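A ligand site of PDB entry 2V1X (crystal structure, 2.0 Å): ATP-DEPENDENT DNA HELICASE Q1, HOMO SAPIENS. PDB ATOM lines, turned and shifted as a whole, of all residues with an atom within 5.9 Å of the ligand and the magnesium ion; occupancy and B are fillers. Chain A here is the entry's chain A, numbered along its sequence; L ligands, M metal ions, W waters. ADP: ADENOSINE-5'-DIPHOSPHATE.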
ATOM      1  N   LEU A  36      -8.278  -3.596  18.597  1.00  0.00           N
ATOM      2  CA  LEU A  36      -9.545  -2.905  18.906  1.00  0.00           C
ATOM      3  C   LEU A  36      -9.756  -1.731  17.932  1.00  0.00           C
ATOM      4  O   LEU A  36     -10.779  -1.632  17.213  1.00  0.00           O
ATOM      5  CB  LEU A  36      -9.545  -2.375  20.388  1.00  0.00           C
ATOM      6  CG  LEU A  36     -10.817  -1.677  20.933  1.00  0.00           C
ATOM      7  CD1 LEU A  36     -12.047  -2.566  21.164  1.00  0.00           C
ATOM      8  CD2 LEU A  36     -10.526  -0.911  22.225  1.00  0.00           C
ATOM      9  N   LEU A  42     -13.193   0.236  16.770  1.00  0.00           N
ATOM     10  CA  LEU A  42     -13.800   0.702  18.008  1.00  0.00           C
ATOM     11  C   LEU A  42     -12.745   1.451  18.723  1.00  0.00           C
ATOM     12  O   LEU A  42     -11.574   1.176  18.563  1.00  0.00           O
ATOM     13  CB  LEU A  42     -14.254  -0.483  18.866  1.00  0.00           C
ATOM     14  CG  LEU A  42     -15.308  -1.350  18.186  1.00  0.00           C
ATOM     15  CD1 LEU A  42     -15.448  -2.695  18.901  1.00  0.00           C
ATOM     16  CD2 LEU A  42     -16.630  -0.584  18.127  1.00  0.00           C
ATOM     17  N   GLU A  43     -13.162   2.394  19.554  1.00  0.00           N
ATOM     18  CA  GLU A  43     -12.231   3.313  20.138  1.00  0.00           C
ATOM     19  C   GLU A  43     -11.870   2.956  21.542  1.00  0.00           C
ATOM     20  O   GLU A  43     -10.710   3.075  21.908  1.00  0.00           O
ATOM     21  CB  GLU A  43     -12.859   4.699  20.131  1.00  0.00           C
ATOM     22  CG  GLU A  43     -11.875   5.790  20.446  1.00  0.00           C
ATOM     23  CD  GLU A  43     -12.517   7.134  20.262  1.00  0.00           C
ATOM     24  OE1 GLU A  43     -13.415   7.453  21.082  1.00  0.00           O
ATOM     25  OE2 GLU A  43     -12.152   7.825  19.280  1.00  0.00           O
ATOM     26  N   LYS A  44     -12.872   2.570  22.340  1.00  0.00           N
ATOM     27  CA  LYS A  44     -12.656   2.193  23.733  1.00  0.00           C
ATOM     28  C   LYS A  44     -13.482   0.959  24.094  1.00  0.00           C
ATOM     29  O   LYS A  44     -14.328   0.524  23.298  1.00  0.00           O
ATOM     30  CB  LYS A  44     -12.988   3.355  24.673  1.00  0.00           C
ATOM     31  CG  LYS A  44     -14.368   3.942  24.495  1.00  0.00           C
ATOM     32  N   PHE A  45     -13.182   0.398  25.259  1.00  0.00           N
ATOM     33  CA  PHE A  45     -13.862  -0.776  25.800  1.00  0.00           C
ATOM     34  C   PHE A  45     -15.031  -0.336  26.667  1.00  0.00           C
ATOM     35  O   PHE A  45     -14.934   0.637  27.426  1.00  0.00           O
ATOM     36  CB  PHE A  45     -12.905  -1.595  26.686  1.00  0.00           C
ATOM     37  CG  PHE A  45     -11.896  -2.405  25.929  1.00  0.00           C
ATOM     38  CD1 PHE A  45     -10.541  -2.090  25.975  1.00  0.00           C
ATOM     39  CD2 PHE A  45     -12.286  -3.475  25.168  1.00  0.00           C
ATOM     40  CE1 PHE A  45      -9.601  -2.845  25.286  1.00  0.00           C
ATOM     41  CE2 PHE A  45     -11.359  -4.232  24.471  1.00  0.00           C
ATOM     42  CZ  PHE A  45     -10.009  -3.925  24.539  1.00  0.00           C
ATOM     43  N   ARG A  46     -16.154  -1.040  26.544  1.00  0.00           N
ATOM     44  CA  ARG A  46     -17.299  -0.847  27.439  1.00  0.00           C
ATOM     45  C   ARG A  46     -17.009  -1.476  28.799  1.00  0.00           C
ATOM     46  O   ARG A  46     -16.050  -2.222  28.937  1.00  0.00           O
ATOM     47  CB  ARG A  46     -18.533  -1.485  26.816  1.00  0.00           C
ATOM     48  CG  ARG A  46     -18.996  -0.723  25.636  1.00  0.00           C
ATOM     49  CD  ARG A  46     -20.046  -1.446  24.896  1.00  0.00           C
ATOM     50  NE  ARG A  46     -20.715  -0.543  23.984  1.00  0.00           N
ATOM     51  CZ  ARG A  46     -21.599  -0.924  23.065  1.00  0.00           C
ATOM     52  NH1 ARG A  46     -21.931  -2.200  22.925  1.00  0.00           N
ATOM     53  NH2 ARG A  46     -22.152  -0.021  22.274  1.00  0.00           N
ATOM     54  N   GLN A  49     -15.367  -5.233  29.411  1.00  0.00           N
ATOM     55  CA  GLN A  49     -14.852  -5.864  28.192  1.00  0.00           C
ATOM     56  C   GLN A  49     -13.343  -6.093  28.258  1.00  0.00           C
ATOM     57  O   GLN A  49     -12.839  -7.128  27.792  1.00  0.00           O
ATOM     58  CB  GLN A  49     -15.166  -5.051  26.946  1.00  0.00           C
ATOM     59  CG  GLN A  49     -16.577  -5.186  26.394  1.00  0.00           C
ATOM     60  CD  GLN A  49     -16.696  -4.482  25.084  1.00  0.00           C
ATOM     61  OE1 GLN A  49     -16.024  -3.469  24.884  1.00  0.00           O
ATOM     62  NE2 GLN A  49     -17.463  -5.029  24.153  1.00  0.00           N
ATOM     63  N   MET A  66     -23.638  -9.999  30.932  1.00  0.00           N
ATOM     64  CA  MET A  66     -23.784  -8.667  30.417  1.00  0.00           C
ATOM     65  C   MET A  66     -25.012  -8.579  29.535  1.00  0.00           C
ATOM     66  O   MET A  66     -25.258  -9.467  28.712  1.00  0.00           O
ATOM     67  CB  MET A  66     -22.554  -8.354  29.574  1.00  0.00           C
ATOM     68  CG  MET A  66     -22.676  -7.120  28.647  1.00  0.00           C
ATOM     69  SD  MET A  66     -21.086  -6.847  27.811  1.00  0.00           S
ATOM     70  CE  MET A  66     -20.059  -6.593  29.284  1.00  0.00           C
ATOM     71  N   PRO A  67     -25.784  -7.475  29.684  1.00  0.00           N
ATOM     72  CA  PRO A  67     -27.021  -7.272  28.932  1.00  0.00           C
ATOM     73  C   PRO A  67     -26.889  -7.563  27.435  1.00  0.00           C
ATOM     74  O   PRO A  67     -25.829  -7.468  26.879  1.00  0.00           O
ATOM     75  CB  PRO A  67     -27.334  -5.806  29.192  1.00  0.00           C
ATOM     76  CG  PRO A  67     -26.729  -5.541  30.540  1.00  0.00           C
ATOM     77  CD  PRO A  67     -25.528  -6.368  30.651  1.00  0.00           C
ATOM     78  N   THR A  68     -27.981  -7.932  26.801  1.00  0.00           N
ATOM     79  CA  THR A  68     -27.956  -8.175  25.339  1.00  0.00           C
ATOM     80  C   THR A  68     -27.674  -6.864  24.611  1.00  0.00           C
ATOM     81  O   THR A  68     -28.195  -5.830  24.988  1.00  0.00           O
ATOM     82  CB  THR A  68     -29.284  -8.750  24.869  1.00  0.00           C
ATOM     83  OG1 THR A  68     -29.519  -9.985  25.537  1.00  0.00           O
ATOM     84  CG2 THR A  68     -29.279  -9.000  23.360  1.00  0.00           C
ATOM     85  N   GLY A  69     -26.874  -6.936  23.541  1.00  0.00           N
ATOM     86  CA  GLY A  69     -26.369  -5.740  22.837  1.00  0.00           C
ATOM     87  C   GLY A  69     -25.239  -4.969  23.524  1.00  0.00           C
ATOM     88  O   GLY A  69     -24.810  -3.935  23.030  1.00  0.00           O
ATOM     89  N   GLY A  70     -24.755  -5.453  24.654  1.00  0.00           N
ATOM     90  CA  GLY A  70     -23.694  -4.781  25.388  1.00  0.00           C
ATOM     91  C   GLY A  70     -22.266  -5.008  24.833  1.00  0.00           C
ATOM     92  O   GLY A  70     -21.371  -4.269  25.201  1.00  0.00           O
ATOM     93  N   GLY A  71     -22.060  -5.989  23.955  1.00  0.00           N
ATOM     94  CA  GLY A  71     -20.740  -6.332  23.406  1.00  0.00           C
ATOM     95  C   GLY A  71     -20.047  -7.551  24.025  1.00  0.00           C
ATOM     96  O   GLY A  71     -18.866  -7.492  24.385  1.00  0.00           O
ATOM     97  N   LYS A  72     -20.773  -8.662  24.187  1.00  0.00           N
ATOM     98  CA  LYS A  72     -20.127  -9.883  24.724  1.00  0.00           C
ATOM     99  C   LYS A  72     -19.196 -10.495  23.709  1.00  0.00           C
ATOM    100  O   LYS A  72     -18.161 -11.020  24.060  1.00  0.00           O
ATOM    101  CB  LYS A  72     -21.161 -10.923  25.202  1.00  0.00           C
ATOM    102  CG  LYS A  72     -21.881 -10.434  26.438  1.00  0.00           C
ATOM    103  CD  LYS A  72     -22.855 -11.449  27.015  1.00  0.00           C
ATOM    104  CE  LYS A  72     -24.179 -11.540  26.287  1.00  0.00           C
ATOM    105  NZ  LYS A  72     -25.023 -10.344  26.398  1.00  0.00           N
ATOM    106  N   SER A  73     -19.572 -10.416  22.437  1.00  0.00           N
ATOM    107  CA  SER A  73     -18.852 -11.121  21.424  1.00  0.00           C
ATOM    108  C   SER A  73     -17.422 -10.671  21.304  1.00  0.00           C
ATOM    109  O   SER A  73     -16.527 -11.481  21.103  1.00  0.00           O
ATOM    110  CB  SER A  73     -19.557 -10.924  20.108  1.00  0.00           C
ATOM    111  OG  SER A  73     -20.909 -11.272  20.281  1.00  0.00           O
ATOM    112  N   LEU A  74     -17.211  -9.366  21.402  1.00  0.00           N
ATOM    113  CA  LEU A  74     -15.889  -8.807  21.320  1.00  0.00           C
ATOM    114  C   LEU A  74     -14.953  -9.566  22.213  1.00  0.00           C
ATOM    115  O   LEU A  74     -13.810  -9.835  21.863  1.00  0.00           O
ATOM    116  CB  LEU A  74     -15.884  -7.309  21.700  1.00  0.00           C
ATOM    117  CG  LEU A  74     -14.599  -6.550  21.363  1.00  0.00           C
ATOM    118  CD1 LEU A  74     -14.301  -6.558  19.879  1.00  0.00           C
ATOM    119  CD2 LEU A  74     -14.683  -5.177  21.838  1.00  0.00           C
ATOM    120  N   TYR A  76     -14.464 -12.479  23.010  1.00  0.00           N
ATOM    121  CA  TYR A  76     -13.792 -13.662  22.500  1.00  0.00           C
ATOM    122  C   TYR A  76     -13.350 -13.496  21.048  1.00  0.00           C
ATOM    123  O   TYR A  76     -12.432 -14.160  20.628  1.00  0.00           O
ATOM    124  CB  TYR A  76     -14.616 -14.965  22.705  1.00  0.00           C
ATOM    125  CG  TYR A  76     -15.938 -14.952  22.004  1.00  0.00           C
ATOM    126  CD1 TYR A  76     -16.014 -15.208  20.646  1.00  0.00           C
ATOM    127  CD2 TYR A  76     -17.109 -14.686  22.679  1.00  0.00           C
ATOM    128  CE1 TYR A  76     -17.190 -15.178  20.017  1.00  0.00           C
ATOM    129  CE2 TYR A  76     -18.286 -14.626  22.047  1.00  0.00           C
ATOM    130  CZ  TYR A  76     -18.329 -14.879  20.702  1.00  0.00           C
ATOM    131  OH  TYR A  76     -19.547 -14.841  20.070  1.00  0.00           O
ATOM    132  N   LEU A  96     -27.889 -16.570  14.936  1.00  0.00           N
ATOM    133  CA  LEU A  96     -26.923 -15.908  15.803  1.00  0.00           C
ATOM    134  C   LEU A  96     -25.494 -16.021  15.274  1.00  0.00           C
ATOM    135  O   LEU A  96     -24.730 -15.053  15.330  1.00  0.00           O
ATOM    136  CB  LEU A  96     -26.991 -16.469  17.224  1.00  0.00           C
ATOM    137  CG  LEU A  96     -28.185 -16.012  18.073  1.00  0.00           C
ATOM    138  CD1 LEU A  96     -28.146 -16.642  19.452  1.00  0.00           C
ATOM    139  CD2 LEU A  96     -28.214 -14.498  18.180  1.00  0.00           C
ATOM    140  N   GLN A 100     -22.948 -12.962  13.399  1.00  0.00           N
ATOM    141  CA  GLN A 100     -21.549 -12.730  13.755  1.00  0.00           C
ATOM    142  C   GLN A 100     -20.636 -12.732  12.542  1.00  0.00           C
ATOM    143  O   GLN A 100     -19.783 -11.872  12.409  1.00  0.00           O
ATOM    144  CB  GLN A 100     -21.080 -13.810  14.709  1.00  0.00           C
ATOM    145  CG  GLN A 100     -21.840 -13.870  16.013  1.00  0.00           C
ATOM    146  CD  GLN A 100     -21.258 -12.989  17.039  1.00  0.00           C
ATOM    147  OE1 GLN A 100     -20.765 -13.455  18.062  1.00  0.00           O
ATOM    148  NE2 GLN A 100     -21.263 -11.680  16.767  1.00  0.00           N
ATOM    149  N   VAL A 103     -20.563  -9.633  10.236  1.00  0.00           N
ATOM    150  CA  VAL A 103     -19.789  -8.565  10.872  1.00  0.00           C
ATOM    151  C   VAL A 103     -18.284  -8.766  10.761  1.00  0.00           C
ATOM    152  O   VAL A 103     -17.548  -7.788  10.574  1.00  0.00           O
ATOM    153  CB  VAL A 103     -20.168  -8.448  12.378  1.00  0.00           C
ATOM    154  CG1 VAL A 103     -19.149  -7.594  13.138  1.00  0.00           C
ATOM    155  CG2 VAL A 103     -21.557  -7.885  12.512  1.00  0.00           C
ATOM    156  N   ASP A 172     -21.261 -19.543  23.507  1.00  0.00           N
ATOM    157  CA  ASP A 172     -22.251 -18.471  23.580  1.00  0.00           C
ATOM    158  C   ASP A 172     -23.521 -19.019  24.236  1.00  0.00           C
ATOM    159  O   ASP A 172     -23.835 -20.193  24.100  1.00  0.00           O
ATOM    160  CB  ASP A 172     -22.552 -17.853  22.213  1.00  0.00           C
ATOM    161  CG  ASP A 172     -22.622 -16.317  22.273  1.00  0.00           C
ATOM    162  OD1 ASP A 172     -22.874 -15.737  23.366  1.00  0.00           O
ATOM    163  OD2 ASP A 172     -22.402 -15.714  21.218  1.00  0.00           O
ATOM    164  N   GLU A 173     -24.205 -18.161  24.996  1.00  0.00           N
ATOM    165  CA  GLU A 173     -25.459 -18.505  25.663  1.00  0.00           C
ATOM    166  C   GLU A 173     -25.274 -19.599  26.724  1.00  0.00           C
ATOM    167  O   GLU A 173     -26.061 -20.514  26.872  1.00  0.00           O
ATOM    168  CB  GLU A 173     -26.536 -18.900  24.639  1.00  0.00           C
ATOM    169  CG  GLU A 173     -26.593 -18.006  23.363  1.00  0.00           C
ATOM    170  CD  GLU A 173     -26.919 -16.532  23.615  1.00  0.00           C
ATOM    171  OE1 GLU A 173     -27.470 -16.213  24.697  1.00  0.00           O
ATOM    172  OE2 GLU A 173     -26.623 -15.704  22.721  1.00  0.00           O
ATOM    173  N   ASP A 332     -28.628  -3.841  16.476  1.00  0.00           N
ATOM    174  CA  ASP A 332     -27.551  -3.105  17.148  1.00  0.00           C
ATOM    175  C   ASP A 332     -27.414  -1.638  16.694  1.00  0.00           C
ATOM    176  O   ASP A 332     -26.388  -0.990  16.987  1.00  0.00           O
ATOM    177  CB  ASP A 332     -26.214  -3.846  16.975  1.00  0.00           C
ATOM    178  CG  ASP A 332     -25.763  -3.953  15.526  1.00  0.00           C
ATOM    179  OD1 ASP A 332     -24.544  -4.044  15.281  1.00  0.00           O
ATOM    180  OD2 ASP A 332     -26.623  -3.977  14.627  1.00  0.00           O
HETATM  181  PB  ADP L   1     -24.138  -9.170  22.871  1.00  0.00           P
HETATM  182  O1B ADP L   1     -25.629  -9.053  22.620  1.00  0.00           O
HETATM  183  O2B ADP L   1     -23.595 -10.451  22.357  1.00  0.00           O
HETATM  184  O3B ADP L   1     -23.688  -8.744  24.289  1.00  0.00           O
HETATM  185  PA  ADP L   1     -22.626  -7.949  20.715  1.00  0.00           P
HETATM  186  O1A ADP L   1     -21.324  -8.596  21.102  1.00  0.00           O
HETATM  187  O2A ADP L   1     -23.327  -8.424  19.516  1.00  0.00           O
HETATM  188  O3A ADP L   1     -23.607  -7.944  21.993  1.00  0.00           O
HETATM  189  O5' ADP L   1     -22.450  -6.378  20.529  1.00  0.00           O
HETATM  190  C5' ADP L   1     -23.542  -5.531  20.199  1.00  0.00           C
HETATM  191  C4' ADP L   1     -23.017  -4.292  19.505  1.00  0.00           C
HETATM  192  O4' ADP L   1     -22.111  -3.578  20.336  1.00  0.00           O
HETATM  193  C3' ADP L   1     -22.270  -4.634  18.224  1.00  0.00           C
HETATM  194  O3' ADP L   1     -22.741  -3.788  17.168  1.00  0.00           O
HETATM  195  C2' ADP L   1     -20.812  -4.390  18.568  1.00  0.00           C
HETATM  196  O2' ADP L   1     -20.043  -4.112  17.397  1.00  0.00           O
HETATM  197  C1' ADP L   1     -20.949  -3.240  19.564  1.00  0.00           C
HETATM  198  N9  ADP L   1     -19.814  -3.087  20.485  1.00  0.00           N
HETATM  199  C8  ADP L   1     -19.197  -4.060  21.169  1.00  0.00           C
HETATM  200  N7  ADP L   1     -18.197  -3.560  21.928  1.00  0.00           N
HETATM  201  C5  ADP L   1     -18.160  -2.241  21.718  1.00  0.00           C
HETATM  202  C6  ADP L   1     -17.330  -1.110  22.181  1.00  0.00           C
HETATM  203  N6  ADP L   1     -16.346  -1.345  23.048  1.00  0.00           N
HETATM  204  N1  ADP L   1     -17.613   0.132  21.736  1.00  0.00           N
HETATM  205  C2  ADP L   1     -18.619   0.355  20.864  1.00  0.00           C
HETATM  206  N3  ADP L   1     -19.415  -0.625  20.386  1.00  0.00           N
HETATM  207  C4  ADP L   1     -19.246  -1.922  20.768  1.00  0.00           C
HETATM  208 MG    MG M   1     -24.228 -12.062  21.672  1.00  0.00          MG
HETATM  209  O   HOH W   1     -15.713   2.480  21.577  1.00  0.00           O
HETATM  210  O   HOH W   2     -24.307 -13.254  23.136  1.00  0.00           O
HETATM  211  O   HOH W   3     -27.026  -8.048  20.624  1.00  0.00           O
HETATM  212  O   HOH W   4     -25.115 -13.797  20.560  1.00  0.00           O
HETATM  213  O   HOH W   5     -22.292 -12.877  21.527  1.00  0.00           O
HETATM  214  O   HOH W   6     -19.139  -7.319  20.452  1.00  0.00           O
HETATM  215  O   HOH W   7     -26.630 -11.691  22.119  1.00  0.00           O
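Leu 42 touches the ligand (CD2 to C2, 3.5 Å).
Phe 45 touches the ligand (CA to N6, 3.8 Å).
Pro 67 touches the ligand.
Thr 68 touches the ligand (C to O1B, 3.6 Å).
CD2 of Leu 74 touches N7 of the ligand, at 3.9 Å.
14 residues have an atom within 4 Å of the ligand: Leu 42, Lys 44, Phe 45, Arg 46, Gln 49, Pro 67, Thr 68, Gly 69, Gly 70, Gly 71, Lys 72, Ser 73, Leu 74 and Asp 332.
The nearest printed residue that does not touch the ligand is Gln 100 (4.7 Å).
Merely in contact with the magnesium ion: Ser 73 (3.7 Å).
Of the 23 residues printed, 1 comes within 4 Å of the magnesium ion.
The nearest printed residue that does not touch the magnesium ion is Asp 172 (4.1 Å).
NH1 of Arg 46 sits at hydrogen-bond distance from O of Gly 69.
N of Arg 46 sits at hydrogen-bond distance from OE1 of Gln 49, 2.9 Å away.
NE2 of Gln 49 sits at hydrogen-bond distance from O of Gly 71, at 2.8 Å.
OE1 of Gln 100 is in hydrogen-bond range of OG of Ser 73 (3.1 Å).
The side-chain amino group (NZ) of Lys 72 is in hydrogen-bond range of the backbone carbonyl oxygen (O) of Pro 67 (3.0 Å).
The backbone carbonyl oxygen of Met 66 is in hydrogen-bond range of the side-chain amino group of Lys 72 (2.5 Å).
The guanidinium group (NH1) of Arg 46 is in hydrogen-bond range of the backbone carbonyl oxygen (O) of Gly 70 (3.1 Å).
N of Leu 42 sits at hydrogen-bond distance from O of Leu 36 (3.1 Å).
Water W4 bridges the side-chain carboxylate of Glu 173 (3.3 Å) and the side-chain carboxylate of Asp 172 (3.4 Å).
Water W5 bridges the side-chain hydroxyl (OG) of Ser 73 and the side-chain carboxylate (OD2) of Asp 172.
Water W2 bridges OD1 of Asp 172 and OE2 of Glu 173.
Water W6 bridges an oxygen (O1A) of the ligand (2.6 Å) and the backbone NH (N) of Leu 74 (3.0 Å).
Water W3 bridges O1B of the ligand (2.6 Å) and N of Gly 69 (3.1 Å).
Water W1 lies within hydrogen-bond range of the backbone NH of Lys 44 (2.9 Å), a nitrogen (N1) of the ligand (3.0 Å) and the backbone NH of Glu 43 (3.3 Å).
The magnesium ion is bound by O2B of the ligand (1.9 Å), water W2 (1.9 Å), water W5 (2.1 Å), water W4 (2.2 Å) and water W7 (2.5 Å).
The side-chain carboxylate of Asp 332 lies within hydrogen-bond range of an oxygen (O3') of the ligand, 2.6 Å away.
The backbone NH of Gly 69 sits at hydrogen-bond distance from an oxygen (O1B) of the ligand, 2.6 Å away.
A nitrogen (N6) of the ligand lies within hydrogen-bond range of the backbone carbonyl oxygen of Lys 44.
A nitrogen (N7) of the ligand lies within hydrogen-bond range of the side-chain amide nitrogen of Gln 49 (2.8 Å).
N of Ser 73 lies within hydrogen-bond range of O1A of the ligand, 2.9 Å away.
An oxygen (O1A) of the ligand sits at hydrogen-bond distance from the side-chain hydroxyl (OG) of Ser 73, at 2.8 Å.
An oxygen (O3B) of the ligand sits at hydrogen-bond distance from the backbone NH of Lys 72 (2.9 Å).
The side-chain amino group (NZ) of Lys 72 is in salt-bridge range of an oxygen (O3B) of the ligand (3.0 Å).
NH1 of Arg 46 sits at hydrogen-bond distance from O4' of the ligand.
The backbone NH (N) of Gly 71 sits at hydrogen-bond distance from an oxygen (O3A) of the ligand.
An oxygen (O3B) of the ligand sits at hydrogen-bond distance from the backbone NH (N) of Gly 70.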
